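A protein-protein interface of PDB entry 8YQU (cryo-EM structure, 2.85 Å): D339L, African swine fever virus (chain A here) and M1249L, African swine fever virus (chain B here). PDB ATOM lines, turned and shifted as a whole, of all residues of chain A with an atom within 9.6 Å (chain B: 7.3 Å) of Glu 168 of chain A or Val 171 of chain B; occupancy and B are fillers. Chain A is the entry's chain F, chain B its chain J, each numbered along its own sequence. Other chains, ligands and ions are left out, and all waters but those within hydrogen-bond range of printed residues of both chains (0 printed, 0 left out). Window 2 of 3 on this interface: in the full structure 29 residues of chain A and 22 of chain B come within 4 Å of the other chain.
N of His 165 of chain A lies within hydrogen-bond range of O of Ile 285 of chain A (2.9 Å). N of Cys 287 of chain A is in hydrogen-bond range of O of His 165 of chain A, 2.9 Å away. N of Gln 167 of chain A is in hydrogen-bond range of O of Cys 287 of chain A (3.3 Å). OE1 of Glu 168 of chain A is in hydrogen-bond range of OG of Ser 288 of chain A, 2.7 Å away. O of Glu 168 of chain A lies within hydrogen-bond range of N of Ala 289 of chain A, 3.1 Å away. NE2 of Gln 202 of chain B sits at hydrogen-bond distance from O of Phe 172 of chain B (2.7 Å).
Among the printed residues, merely in contact across the chains: Glu 168 of chain A with Val 171 of chain B (3.9 Å), Ile 285 of chain A with Phe 172 of chain B (3.99 Å), Cys 287 of chain A with Val 171 of chain B (3.6 Å), Ser 288 of chain A with Val 171 of chain B (3.0 Å), Val 291 of chain A with Phe 168 of chain B (3.5 Å) and Val 291 of chain A with Phe 172 of chain B (3.6 Å).
The side-chain amide nitrogen of Gln 202 of chain B is in hydrogen-bond range of the backbone carbonyl oxygen of Ile 286 of chain A (2.7 Å).
Of the 12 printed residues of chain B, 4 touch a printed residue of chain A. Hydrophobic or aromatic side chains of chain A that line the printed part of chain B: Ile 285, Ile 286 and Val 291. Among the printed residues, no Asp or Glu carboxylate lies within 4 Å of a Lys or Arg side-chain nitrogen of the other chain.
Glu 168 of chain A touches one residue of chain B. Printed residues of chain B within 4 Å of Ile 286 of chain A: Gln 202. Of the printed residues of chain B, Val 291 of chain A touches Phe 168 (3.5 Å) and Phe 172 (3.6 Å). Met 173 of chain B touches none of the printed residues of chain A. The nearest residue of chain B that does not touch Glu 168 of chain A is Arg 170 of chain B (5.9 Å).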
ATOM      1  N   TYR A 164      -4.650  10.855 -19.043  1.00  0.00           N
ATOM      2  CA  TYR A 164      -5.900  10.111 -18.983  1.00  0.00           C
ATOM      3  C   TYR A 164      -6.011   9.399 -17.641  1.00  0.00           C
ATOM      4  O   TYR A 164      -5.121   8.630 -17.266  1.00  0.00           O
ATOM      5  CB  TYR A 164      -5.984   9.097 -20.126  1.00  0.00           C
ATOM      6  CG  TYR A 164      -5.911   9.711 -21.507  1.00  0.00           C
ATOM      7  CD1 TYR A 164      -6.406  10.985 -21.751  1.00  0.00           C
ATOM      8  CD2 TYR A 164      -5.337   9.020 -22.565  1.00  0.00           C
ATOM      9  CE1 TYR A 164      -6.339  11.548 -23.010  1.00  0.00           C
ATOM     10  CE2 TYR A 164      -5.266   9.576 -23.828  1.00  0.00           C
ATOM     11  CZ  TYR A 164      -5.767  10.840 -24.044  1.00  0.00           C
ATOM     12  OH  TYR A 164      -5.696  11.396 -25.301  1.00  0.00           O
ATOM     13  N   HIS A 165      -7.104   9.657 -16.924  1.00  0.00           N
ATOM     14  CA  HIS A 165      -7.420   8.979 -15.671  1.00  0.00           C
ATOM     15  C   HIS A 165      -8.342   7.809 -15.988  1.00  0.00           C
ATOM     16  O   HIS A 165      -9.541   7.992 -16.217  1.00  0.00           O
ATOM     17  CB  HIS A 165      -8.074   9.935 -14.682  1.00  0.00           C
ATOM     18  CG  HIS A 165      -7.834   9.576 -13.248  1.00  0.00           C
ATOM     19  ND1 HIS A 165      -8.208   8.361 -12.716  1.00  0.00           N
ATOM     20  CD2 HIS A 165      -7.284  10.279 -12.232  1.00  0.00           C
ATOM     21  CE1 HIS A 165      -7.883   8.326 -11.436  1.00  0.00           C
ATOM     22  NE2 HIS A 165      -7.322   9.477 -11.117  1.00  0.00           N
ATOM     23  N   VAL A 166      -7.782   6.604 -15.987  1.00  0.00           N
ATOM     24  CA  VAL A 166      -8.535   5.389 -16.263  1.00  0.00           C
ATOM     25  C   VAL A 166      -8.924   4.722 -14.948  1.00  0.00           C
ATOM     26  O   VAL A 166      -8.087   4.528 -14.059  1.00  0.00           O
ATOM     27  CB  VAL A 166      -7.737   4.438 -17.169  1.00  0.00           C
ATOM     28  CG1 VAL A 166      -6.433   4.042 -16.523  1.00  0.00           C
ATOM     29  CG2 VAL A 166      -8.547   3.193 -17.433  1.00  0.00           C
ATOM     30  N   GLN A 167     -10.212   4.393 -14.822  1.00  0.00           N
ATOM     31  CA  GLN A 167     -10.759   3.757 -13.635  1.00  0.00           C
ATOM     32  C   GLN A 167     -11.448   2.431 -13.919  1.00  0.00           C
ATOM     33  O   GLN A 167     -11.754   1.701 -12.970  1.00  0.00           O
ATOM     34  CB  GLN A 167     -11.758   4.697 -12.939  1.00  0.00           C
ATOM     35  CG  GLN A 167     -11.251   6.118 -12.758  1.00  0.00           C
ATOM     36  CD  GLN A 167     -12.361   7.094 -12.420  1.00  0.00           C
ATOM     37  OE1 GLN A 167     -13.539   6.811 -12.638  1.00  0.00           O
ATOM     38  NE2 GLN A 167     -11.990   8.253 -11.888  1.00  0.00           N
ATOM     39  N   GLU A 168     -11.713   2.105 -15.182  1.00  0.00           N
ATOM     40  CA  GLU A 168     -12.317   0.836 -15.567  1.00  0.00           C
ATOM     41  C   GLU A 168     -11.436   0.172 -16.614  1.00  0.00           C
ATOM     42  O   GLU A 168     -10.953   0.837 -17.535  1.00  0.00           O
ATOM     43  CB  GLU A 168     -13.741   1.034 -16.101  1.00  0.00           C
ATOM     44  CG  GLU A 168     -14.616   1.925 -15.226  1.00  0.00           C
ATOM     45  CD  GLU A 168     -14.602   3.378 -15.658  1.00  0.00           C
ATOM     46  OE1 GLU A 168     -13.516   3.888 -16.005  1.00  0.00           O
ATOM     47  OE2 GLU A 168     -15.679   4.012 -15.653  1.00  0.00           O
ATOM     48  N   GLU A 169     -11.232  -1.134 -16.471  1.00  0.00           N
ATOM     49  CA  GLU A 169     -10.272  -1.869 -17.279  1.00  0.00           C
ATOM     50  C   GLU A 169     -10.980  -2.616 -18.410  1.00  0.00           C
ATOM     51  O   GLU A 169     -12.181  -2.461 -18.646  1.00  0.00           O
ATOM     52  CB  GLU A 169      -9.468  -2.825 -16.396  1.00  0.00           C
ATOM     53  CG  GLU A 169      -8.031  -3.042 -16.851  1.00  0.00           C
ATOM     54  CD  GLU A 169      -7.226  -3.855 -15.859  1.00  0.00           C
ATOM     55  OE1 GLU A 169      -7.250  -3.521 -14.657  1.00  0.00           O
ATOM     56  OE2 GLU A 169      -6.569  -4.829 -16.284  1.00  0.00           O
ATOM     57  N   LEU A 170     -10.212  -3.438 -19.120  1.00  0.00           N
ATOM     58  CA  LEU A 170     -10.704  -4.155 -20.287  1.00  0.00           C
ATOM     59  C   LEU A 170     -11.445  -5.420 -19.878  1.00  0.00           C
ATOM     60  O   LEU A 170     -11.317  -5.907 -18.749  1.00  0.00           O
ATOM     61  CB  LEU A 170      -9.548  -4.549 -21.209  1.00  0.00           C
ATOM     62  CG  LEU A 170      -8.895  -3.555 -22.174  1.00  0.00           C
ATOM     63  CD1 LEU A 170      -9.879  -3.023 -23.204  1.00  0.00           C
ATOM     64  CD2 LEU A 170      -8.217  -2.430 -21.425  1.00  0.00           C
ATOM     65  N   THR A 171     -12.229  -5.953 -20.811  1.00  0.00           N
ATOM     66  CA  THR A 171     -12.683  -7.331 -20.732  1.00  0.00           C
ATOM     67  C   THR A 171     -12.016  -8.130 -21.852  1.00  0.00           C
ATOM     68  O   THR A 171     -11.161  -7.624 -22.582  1.00  0.00           O
ATOM     69  CB  THR A 171     -14.207  -7.420 -20.805  1.00  0.00           C
ATOM     70  OG1 THR A 171     -14.619  -8.762 -20.518  1.00  0.00           O
ATOM     71  CG2 THR A 171     -14.694  -7.054 -22.191  1.00  0.00           C
ATOM     72  N   GLN A 174     -13.085  -6.708 -25.344  1.00  0.00           N
ATOM     73  CA  GLN A 174     -12.517  -5.381 -25.531  1.00  0.00           C
ATOM     74  C   GLN A 174     -11.008  -5.403 -25.742  1.00  0.00           C
ATOM     75  O   GLN A 174     -10.455  -4.405 -26.213  1.00  0.00           O
ATOM     76  CB  GLN A 174     -12.876  -4.491 -24.340  1.00  0.00           C
ATOM     77  CG  GLN A 174     -14.362  -4.204 -24.201  1.00  0.00           C
ATOM     78  CD  GLN A 174     -14.712  -3.567 -22.869  1.00  0.00           C
ATOM     79  OE1 GLN A 174     -13.965  -2.737 -22.349  1.00  0.00           O
ATOM     80  NE2 GLN A 174     -15.857  -3.947 -22.313  1.00  0.00           N
ATOM     81  N   SER A 252      -3.041  -4.800 -14.003  1.00  0.00           N
ATOM     82  CA  SER A 252      -4.105  -3.816 -13.866  1.00  0.00           C
ATOM     83  C   SER A 252      -3.717  -2.524 -14.575  1.00  0.00           C
ATOM     84  O   SER A 252      -2.625  -1.988 -14.359  1.00  0.00           O
ATOM     85  CB  SER A 252      -4.403  -3.532 -12.392  1.00  0.00           C
ATOM     86  OG  SER A 252      -5.451  -2.588 -12.256  1.00  0.00           O
ATOM     87  N   SER A 253      -4.622  -2.022 -15.414  1.00  0.00           N
ATOM     88  CA  SER A 253      -4.355  -0.865 -16.260  1.00  0.00           C
ATOM     89  C   SER A 253      -4.847   0.446 -15.657  1.00  0.00           C
ATOM     90  O   SER A 253      -4.686   1.497 -16.284  1.00  0.00           O
ATOM     91  CB  SER A 253      -4.985  -1.071 -17.640  1.00  0.00           C
ATOM     92  OG  SER A 253      -4.905   0.109 -18.420  1.00  0.00           O
ATOM     93  N   LEU A 254      -5.431   0.414 -14.461  1.00  0.00           N
ATOM     94  CA  LEU A 254      -5.998   1.612 -13.859  1.00  0.00           C
ATOM     95  C   LEU A 254      -4.906   2.614 -13.492  1.00  0.00           C
ATOM     96  O   LEU A 254      -3.750   2.256 -13.245  1.00  0.00           O
ATOM     97  CB  LEU A 254      -6.814   1.253 -12.616  1.00  0.00           C
ATOM     98  CG  LEU A 254      -8.255   0.775 -12.813  1.00  0.00           C
ATOM     99  CD1 LEU A 254      -8.303  -0.636 -13.383  1.00  0.00           C
ATOM    100  CD2 LEU A 254      -9.013   0.846 -11.498  1.00  0.00           C
ATOM    101  N   GLY A 255      -5.286   3.893 -13.459  1.00  0.00           N
ATOM    102  CA  GLY A 255      -4.360   4.933 -13.046  1.00  0.00           C
ATOM    103  C   GLY A 255      -4.246   6.110 -13.994  1.00  0.00           C
ATOM    104  O   GLY A 255      -5.181   6.415 -14.739  1.00  0.00           O
ATOM    105  N   TRP A 257      -2.363   7.755 -17.213  1.00  0.00           N
ATOM    106  CA  TRP A 257      -1.577   7.425 -18.393  1.00  0.00           C
ATOM    107  C   TRP A 257      -1.214   8.695 -19.148  1.00  0.00           C
ATOM    108  O   TRP A 257      -2.031   9.613 -19.271  1.00  0.00           O
ATOM    109  CB  TRP A 257      -2.337   6.470 -19.309  1.00  0.00           C
ATOM    110  CG  TRP A 257      -2.359   5.057 -18.822  1.00  0.00           C
ATOM    111  CD1 TRP A 257      -3.251   4.504 -17.950  1.00  0.00           C
ATOM    112  CD2 TRP A 257      -1.465   4.004 -19.201  1.00  0.00           C
ATOM    113  NE1 TRP A 257      -2.960   3.175 -17.756  1.00  0.00           N
ATOM    114  CE2 TRP A 257      -1.870   2.843 -18.515  1.00  0.00           C
ATOM    115  CE3 TRP A 257      -0.360   3.932 -20.056  1.00  0.00           C
ATOM    116  CZ2 TRP A 257      -1.207   1.627 -18.651  1.00  0.00           C
ATOM    117  CZ3 TRP A 257       0.297   2.722 -20.190  1.00  0.00           C
ATOM    118  CH2 TRP A 257      -0.128   1.587 -19.491  1.00  0.00           C
ATOM    119  N   ILE A 285      -8.207  13.780 -17.922  1.00  0.00           N
ATOM    120  CA  ILE A 285      -9.430  13.395 -18.617  1.00  0.00           C
ATOM    121  C   ILE A 285      -9.926  12.091 -18.003  1.00  0.00           C
ATOM    122  O   ILE A 285      -9.293  11.045 -18.159  1.00  0.00           O
ATOM    123  CB  ILE A 285      -9.189  13.248 -20.122  1.00  0.00           C
ATOM    124  CG1 ILE A 285      -8.747  14.587 -20.715  1.00  0.00           C
ATOM    125  CG2 ILE A 285     -10.443  12.741 -20.816  1.00  0.00           C
ATOM    126  CD1 ILE A 285      -8.068  14.463 -22.057  1.00  0.00           C
ATOM    127  N   ILE A 286     -11.052  12.155 -17.296  1.00  0.00           N
ATOM    128  CA  ILE A 286     -11.620  10.976 -16.647  1.00  0.00           C
ATOM    129  C   ILE A 286     -12.255  10.091 -17.709  1.00  0.00           C
ATOM    130  O   ILE A 286     -13.068  10.561 -18.516  1.00  0.00           O
ATOM    131  CB  ILE A 286     -12.648  11.384 -15.581  1.00  0.00           C
ATOM    132  CG1 ILE A 286     -12.084  12.477 -14.672  1.00  0.00           C
ATOM    133  CG2 ILE A 286     -13.077  10.172 -14.766  1.00  0.00           C
ATOM    134  CD1 ILE A 286     -10.814  12.091 -13.955  1.00  0.00           C
ATOM    135  N   CYS A 287     -11.904   8.808 -17.708  1.00  0.00           N
ATOM    136  CA  CYS A 287     -12.317   7.911 -18.780  1.00  0.00           C
ATOM    137  C   CYS A 287     -11.992   6.476 -18.379  1.00  0.00           C
ATOM    138  O   CYS A 287     -11.502   6.215 -17.275  1.00  0.00           O
ATOM    139  CB  CYS A 287     -11.629   8.309 -20.087  1.00  0.00           C
ATOM    140  SG  CYS A 287      -9.840   8.037 -20.075  1.00  0.00           S
ATOM    141  N   SER A 288     -12.273   5.539 -19.281  1.00  0.00           N
ATOM    142  CA  SER A 288     -11.913   4.135 -19.137  1.00  0.00           C
ATOM    143  C   SER A 288     -10.683   3.823 -19.980  1.00  0.00           C
ATOM    144  O   SER A 288     -10.037   4.710 -20.545  1.00  0.00           O
ATOM    145  CB  SER A 288     -13.074   3.218 -19.528  1.00  0.00           C
ATOM    146  OG  SER A 288     -14.128   3.277 -18.587  1.00  0.00           O
ATOM    147  N   ALA A 289     -10.362   2.531 -20.057  1.00  0.00           N
ATOM    148  CA  ALA A 289      -9.171   2.101 -20.775  1.00  0.00           C
ATOM    149  C   ALA A 289      -9.408   1.958 -22.271  1.00  0.00           C
ATOM    150  O   ALA A 289      -8.444   2.002 -23.040  1.00  0.00           O
ATOM    151  CB  ALA A 289      -8.658   0.786 -20.193  1.00  0.00           C
ATOM    152  N   GLU A 290     -10.661   1.790 -22.700  1.00  0.00           N
ATOM    153  CA  GLU A 290     -10.957   1.718 -24.128  1.00  0.00           C
ATOM    154  C   GLU A 290     -10.462   2.958 -24.860  1.00  0.00           C
ATOM    155  O   GLU A 290      -9.718   2.862 -25.843  1.00  0.00           O
ATOM    156  CB  GLU A 290     -12.461   1.536 -24.343  1.00  0.00           C
ATOM    157  CG  GLU A 290     -12.924   0.104 -24.243  1.00  0.00           C
ATOM    158  CD  GLU A 290     -12.588  -0.675 -25.497  1.00  0.00           C
ATOM    159  OE1 GLU A 290     -12.883  -0.174 -26.604  1.00  0.00           O
ATOM    160  OE2 GLU A 290     -12.005  -1.768 -25.385  1.00  0.00           O
ATOM    161  N   VAL A 291     -10.858   4.137 -24.380  1.00  0.00           N
ATOM    162  CA  VAL A 291     -10.559   5.365 -25.105  1.00  0.00           C
ATOM    163  C   VAL A 291      -9.059   5.642 -25.094  1.00  0.00           C
ATOM    164  O   VAL A 291      -8.476   5.995 -26.125  1.00  0.00           O
ATOM    165  CB  VAL A 291     -11.370   6.537 -24.522  1.00  0.00           C
ATOM    166  CG1 VAL A 291     -12.853   6.261 -24.654  1.00  0.00           C
ATOM    167  CG2 VAL A 291     -11.032   6.755 -23.078  1.00  0.00           C
ATOM    168  N   MET A 292      -8.406   5.467 -23.943  1.00  0.00           N
ATOM    169  CA  MET A 292      -6.978   5.747 -23.865  1.00  0.00           C
ATOM    170  C   MET A 292      -6.174   4.752 -24.694  1.00  0.00           C
ATOM    171  O   MET A 292      -5.229   5.137 -25.393  1.00  0.00           O
ATOM    172  CB  MET A 292      -6.514   5.770 -22.406  1.00  0.00           C
ATOM    173  CG  MET A 292      -6.740   4.500 -21.610  1.00  0.00           C
ATOM    174  SD  MET A 292      -5.575   3.182 -21.982  1.00  0.00           S
ATOM    175  CE  MET A 292      -4.064   3.846 -21.321  1.00  0.00           C
ATOM    176  N   PHE A 293      -6.533   3.466 -24.636  1.00  0.00           N
ATOM    177  CA  PHE A 293      -5.827   2.481 -25.449  1.00  0.00           C
ATOM    178  C   PHE A 293      -6.003   2.763 -26.933  1.00  0.00           C
ATOM    179  O   PHE A 293      -5.027   2.739 -27.691  1.00  0.00           O
ATOM    180  CB  PHE A 293      -6.292   1.061 -25.117  1.00  0.00           C
ATOM    181  CG  PHE A 293      -5.482   0.392 -24.041  1.00  0.00           C
ATOM    182  CD1 PHE A 293      -4.151   0.076 -24.262  1.00  0.00           C
ATOM    183  CD2 PHE A 293      -6.050   0.051 -22.827  1.00  0.00           C
ATOM    184  CE1 PHE A 293      -3.396  -0.542 -23.284  1.00  0.00           C
ATOM    185  CE2 PHE A 293      -5.299  -0.564 -21.842  1.00  0.00           C
ATOM    186  CZ  PHE A 293      -3.972  -0.865 -22.073  1.00  0.00           C
ATOM    187  N   LEU B 134     -29.070  10.493 -20.746  1.00  0.00           N
ATOM    188  CA  LEU B 134     -28.531   9.277 -21.348  1.00  0.00           C
ATOM    189  C   LEU B 134     -29.634   8.659 -22.201  1.00  0.00           C
ATOM    190  O   LEU B 134     -30.334   7.731 -21.796  1.00  0.00           O
ATOM    191  CB  LEU B 134     -28.023   8.314 -20.276  1.00  0.00           C
ATOM    192  CG  LEU B 134     -26.584   8.509 -19.785  1.00  0.00           C
ATOM    193  CD1 LEU B 134     -25.604   8.287 -20.926  1.00  0.00           C
ATOM    194  CD2 LEU B 134     -26.371   9.876 -19.147  1.00  0.00           C
ATOM    195  N   ASN B 167     -19.667   1.981 -24.865  1.00  0.00           N
ATOM    196  CA  ASN B 167     -19.612   2.413 -23.470  1.00  0.00           C
ATOM    197  C   ASN B 167     -18.707   3.634 -23.332  1.00  0.00           C
ATOM    198  O   ASN B 167     -17.752   3.651 -22.555  1.00  0.00           O
ATOM    199  CB  ASN B 167     -19.155   1.255 -22.584  1.00  0.00           C
ATOM    200  CG  ASN B 167     -19.148   1.607 -21.108  1.00  0.00           C
ATOM    201  OD1 ASN B 167     -20.046   2.291 -20.618  1.00  0.00           O
ATOM    202  ND2 ASN B 167     -18.136   1.132 -20.391  1.00  0.00           N
ATOM    203  N   PHE B 168     -18.962   4.666 -24.137  1.00  0.00           N
ATOM    204  CA  PHE B 168     -18.128   5.864 -24.134  1.00  0.00           C
ATOM    205  C   PHE B 168     -18.760   7.035 -23.386  1.00  0.00           C
ATOM    206  O   PHE B 168     -18.129   7.615 -22.493  1.00  0.00           O
ATOM    207  CB  PHE B 168     -17.806   6.277 -25.575  1.00  0.00           C
ATOM    208  CG  PHE B 168     -17.047   5.235 -26.345  1.00  0.00           C
ATOM    209  CD1 PHE B 168     -15.780   4.850 -25.948  1.00  0.00           C
ATOM    210  CD2 PHE B 168     -17.596   4.648 -27.471  1.00  0.00           C
ATOM    211  CE1 PHE B 168     -15.075   3.893 -26.653  1.00  0.00           C
ATOM    212  CE2 PHE B 168     -16.896   3.691 -28.183  1.00  0.00           C
ATOM    213  CZ  PHE B 168     -15.634   3.314 -27.772  1.00  0.00           C
ATOM    214  N   ILE B 169     -19.992   7.404 -23.745  1.00  0.00           N
ATOM    215  CA  ILE B 169     -20.650   8.534 -23.091  1.00  0.00           C
ATOM    216  C   ILE B 169     -20.900   8.230 -21.619  1.00  0.00           C
ATOM    217  O   ILE B 169     -20.679   9.081 -20.749  1.00  0.00           O
ATOM    218  CB  ILE B 169     -21.955   8.896 -23.826  1.00  0.00           C
ATOM    219  CG1 ILE B 169     -21.652   9.364 -25.250  1.00  0.00           C
ATOM    220  CG2 ILE B 169     -22.717   9.970 -23.066  1.00  0.00           C
ATOM    221  CD1 ILE B 169     -22.881   9.503 -26.121  1.00  0.00           C
ATOM    222  N   ARG B 170     -21.357   7.013 -21.314  1.00  0.00           N
ATOM    223  CA  ARG B 170     -21.609   6.639 -19.928  1.00  0.00           C
ATOM    224  C   ARG B 170     -20.336   6.622 -19.093  1.00  0.00           C
ATOM    225  O   ARG B 170     -20.418   6.677 -17.861  1.00  0.00           O
ATOM    226  CB  ARG B 170     -22.293   5.272 -19.865  1.00  0.00           C
ATOM    227  CG  ARG B 170     -23.696   5.254 -20.455  1.00  0.00           C
ATOM    228  CD  ARG B 170     -24.302   3.862 -20.415  1.00  0.00           C
ATOM    229  NE  ARG B 170     -24.518   3.393 -19.052  1.00  0.00           N
ATOM    230  CZ  ARG B 170     -25.619   3.621 -18.348  1.00  0.00           C
ATOM    231  NH1 ARG B 170     -26.632   4.307 -18.850  1.00  0.00           N
ATOM    232  NH2 ARG B 170     -25.705   3.150 -17.107  1.00  0.00           N
ATOM    233  N   VAL B 171     -19.170   6.546 -19.727  1.00  0.00           N
ATOM    234  CA  VAL B 171     -17.900   6.585 -19.008  1.00  0.00           C
ATOM    235  C   VAL B 171     -17.397   8.009 -18.829  1.00  0.00           C
ATOM    236  O   VAL B 171     -16.972   8.390 -17.735  1.00  0.00           O
ATOM    237  CB  VAL B 171     -16.852   5.712 -19.723  1.00  0.00           C
ATOM    238  CG1 VAL B 171     -15.508   5.919 -19.077  1.00  0.00           C
ATOM    239  CG2 VAL B 171     -17.242   4.257 -19.607  1.00  0.00           C
ATOM    240  N   PHE B 172     -17.414   8.816 -19.893  1.00  0.00           N
ATOM    241  CA  PHE B 172     -16.940  10.190 -19.752  1.00  0.00           C
ATOM    242  C   PHE B 172     -17.779  10.981 -18.758  1.00  0.00           C
ATOM    243  O   PHE B 172     -17.296  11.970 -18.197  1.00  0.00           O
ATOM    244  CB  PHE B 172     -16.928  10.894 -21.109  1.00  0.00           C
ATOM    245  CG  PHE B 172     -15.682  10.642 -21.906  1.00  0.00           C
ATOM    246  CD1 PHE B 172     -15.418   9.388 -22.428  1.00  0.00           C
ATOM    247  CD2 PHE B 172     -14.763  11.655 -22.116  1.00  0.00           C
ATOM    248  CE1 PHE B 172     -14.270   9.153 -23.158  1.00  0.00           C
ATOM    249  CE2 PHE B 172     -13.612  11.426 -22.845  1.00  0.00           C
ATOM    250  CZ  PHE B 172     -13.366  10.174 -23.367  1.00  0.00           C
ATOM    251  N   MET B 173     -19.017  10.564 -18.531  1.00  0.00           N
ATOM    252  CA  MET B 173     -19.896  11.143 -17.527  1.00  0.00           C
ATOM    253  C   MET B 173     -19.737  10.356 -16.224  1.00  0.00           C
ATOM    254  O   MET B 173     -18.714   9.697 -16.016  1.00  0.00           O
ATOM    255  CB  MET B 173     -21.326  11.199 -18.068  1.00  0.00           C
ATOM    256  CG  MET B 173     -21.420  12.118 -19.270  1.00  0.00           C
ATOM    257  SD  MET B 173     -20.989  13.808 -18.812  1.00  0.00           S
ATOM    258  CE  MET B 173     -20.901  14.595 -20.417  1.00  0.00           C
ATOM    259  N   LYS B 174     -20.716  10.467 -15.319  1.00  0.00           N
ATOM    260  CA  LYS B 174     -20.690   9.890 -13.973  1.00  0.00           C
ATOM    261  C   LYS B 174     -19.787  10.704 -13.054  1.00  0.00           C
ATOM    262  O   LYS B 174     -19.143  10.159 -12.153  1.00  0.00           O
ATOM    263  CB  LYS B 174     -20.257   8.418 -13.983  1.00  0.00           C
ATOM    264  CG  LYS B 174     -21.140   7.471 -14.798  1.00  0.00           C
ATOM    265  CD  LYS B 174     -22.503   7.223 -14.156  1.00  0.00           C
ATOM    266  CE  LYS B 174     -23.584   8.148 -14.699  1.00  0.00           C
ATOM    267  NZ  LYS B 174     -24.924   7.817 -14.140  1.00  0.00           N
ATOM    268  N   CYS B 175     -19.737  12.016 -13.290  1.00  0.00           N
ATOM    269  CA  CYS B 175     -19.149  12.972 -12.360  1.00  0.00           C
ATOM    270  C   CYS B 175     -20.170  13.499 -11.360  1.00  0.00           C
ATOM    271  O   CYS B 175     -20.052  14.641 -10.893  1.00  0.00           O
ATOM    272  CB  CYS B 175     -18.508  14.127 -13.131  1.00  0.00           C
ATOM    273  SG  CYS B 175     -19.682  15.125 -14.077  1.00  0.00           S
ATOM    274  N   GLN B 202     -15.473  17.224 -19.199  1.00  0.00           N
ATOM    275  CA  GLN B 202     -15.742  15.854 -19.620  1.00  0.00           C
ATOM    276  C   GLN B 202     -16.543  15.817 -20.913  1.00  0.00           C
ATOM    277  O   GLN B 202     -16.284  14.980 -21.780  1.00  0.00           O
ATOM    278  CB  GLN B 202     -16.469  15.098 -18.509  1.00  0.00           C
ATOM    279  CG  GLN B 202     -15.602  14.803 -17.298  1.00  0.00           C
ATOM    280  CD  GLN B 202     -14.406  13.934 -17.638  1.00  0.00           C
ATOM    281  OE1 GLN B 202     -13.261  14.383 -17.578  1.00  0.00           O
ATOM    282  NE2 GLN B 202     -14.666  12.684 -18.000  1.00  0.00           N
ATOM    283  N   LEU B 206     -15.284  14.329 -24.340  1.00  0.00           N
ATOM    284  CA  LEU B 206     -16.066  13.244 -24.921  1.00  0.00           C
ATOM    285  C   LEU B 206     -16.258  13.456 -26.415  1.00  0.00           C
ATOM    286  O   LEU B 206     -15.999  12.555 -27.219  1.00  0.00           O
ATOM    287  CB  LEU B 206     -17.415  13.134 -24.210  1.00  0.00           C
ATOM    288  CG  LEU B 206     -18.528  12.377 -24.938  1.00  0.00           C
ATOM    289  CD1 LEU B 206     -18.170  10.907 -25.100  1.00  0.00           C
ATOM    290  CD2 LEU B 206     -19.848  12.533 -24.200  1.00  0.00           C
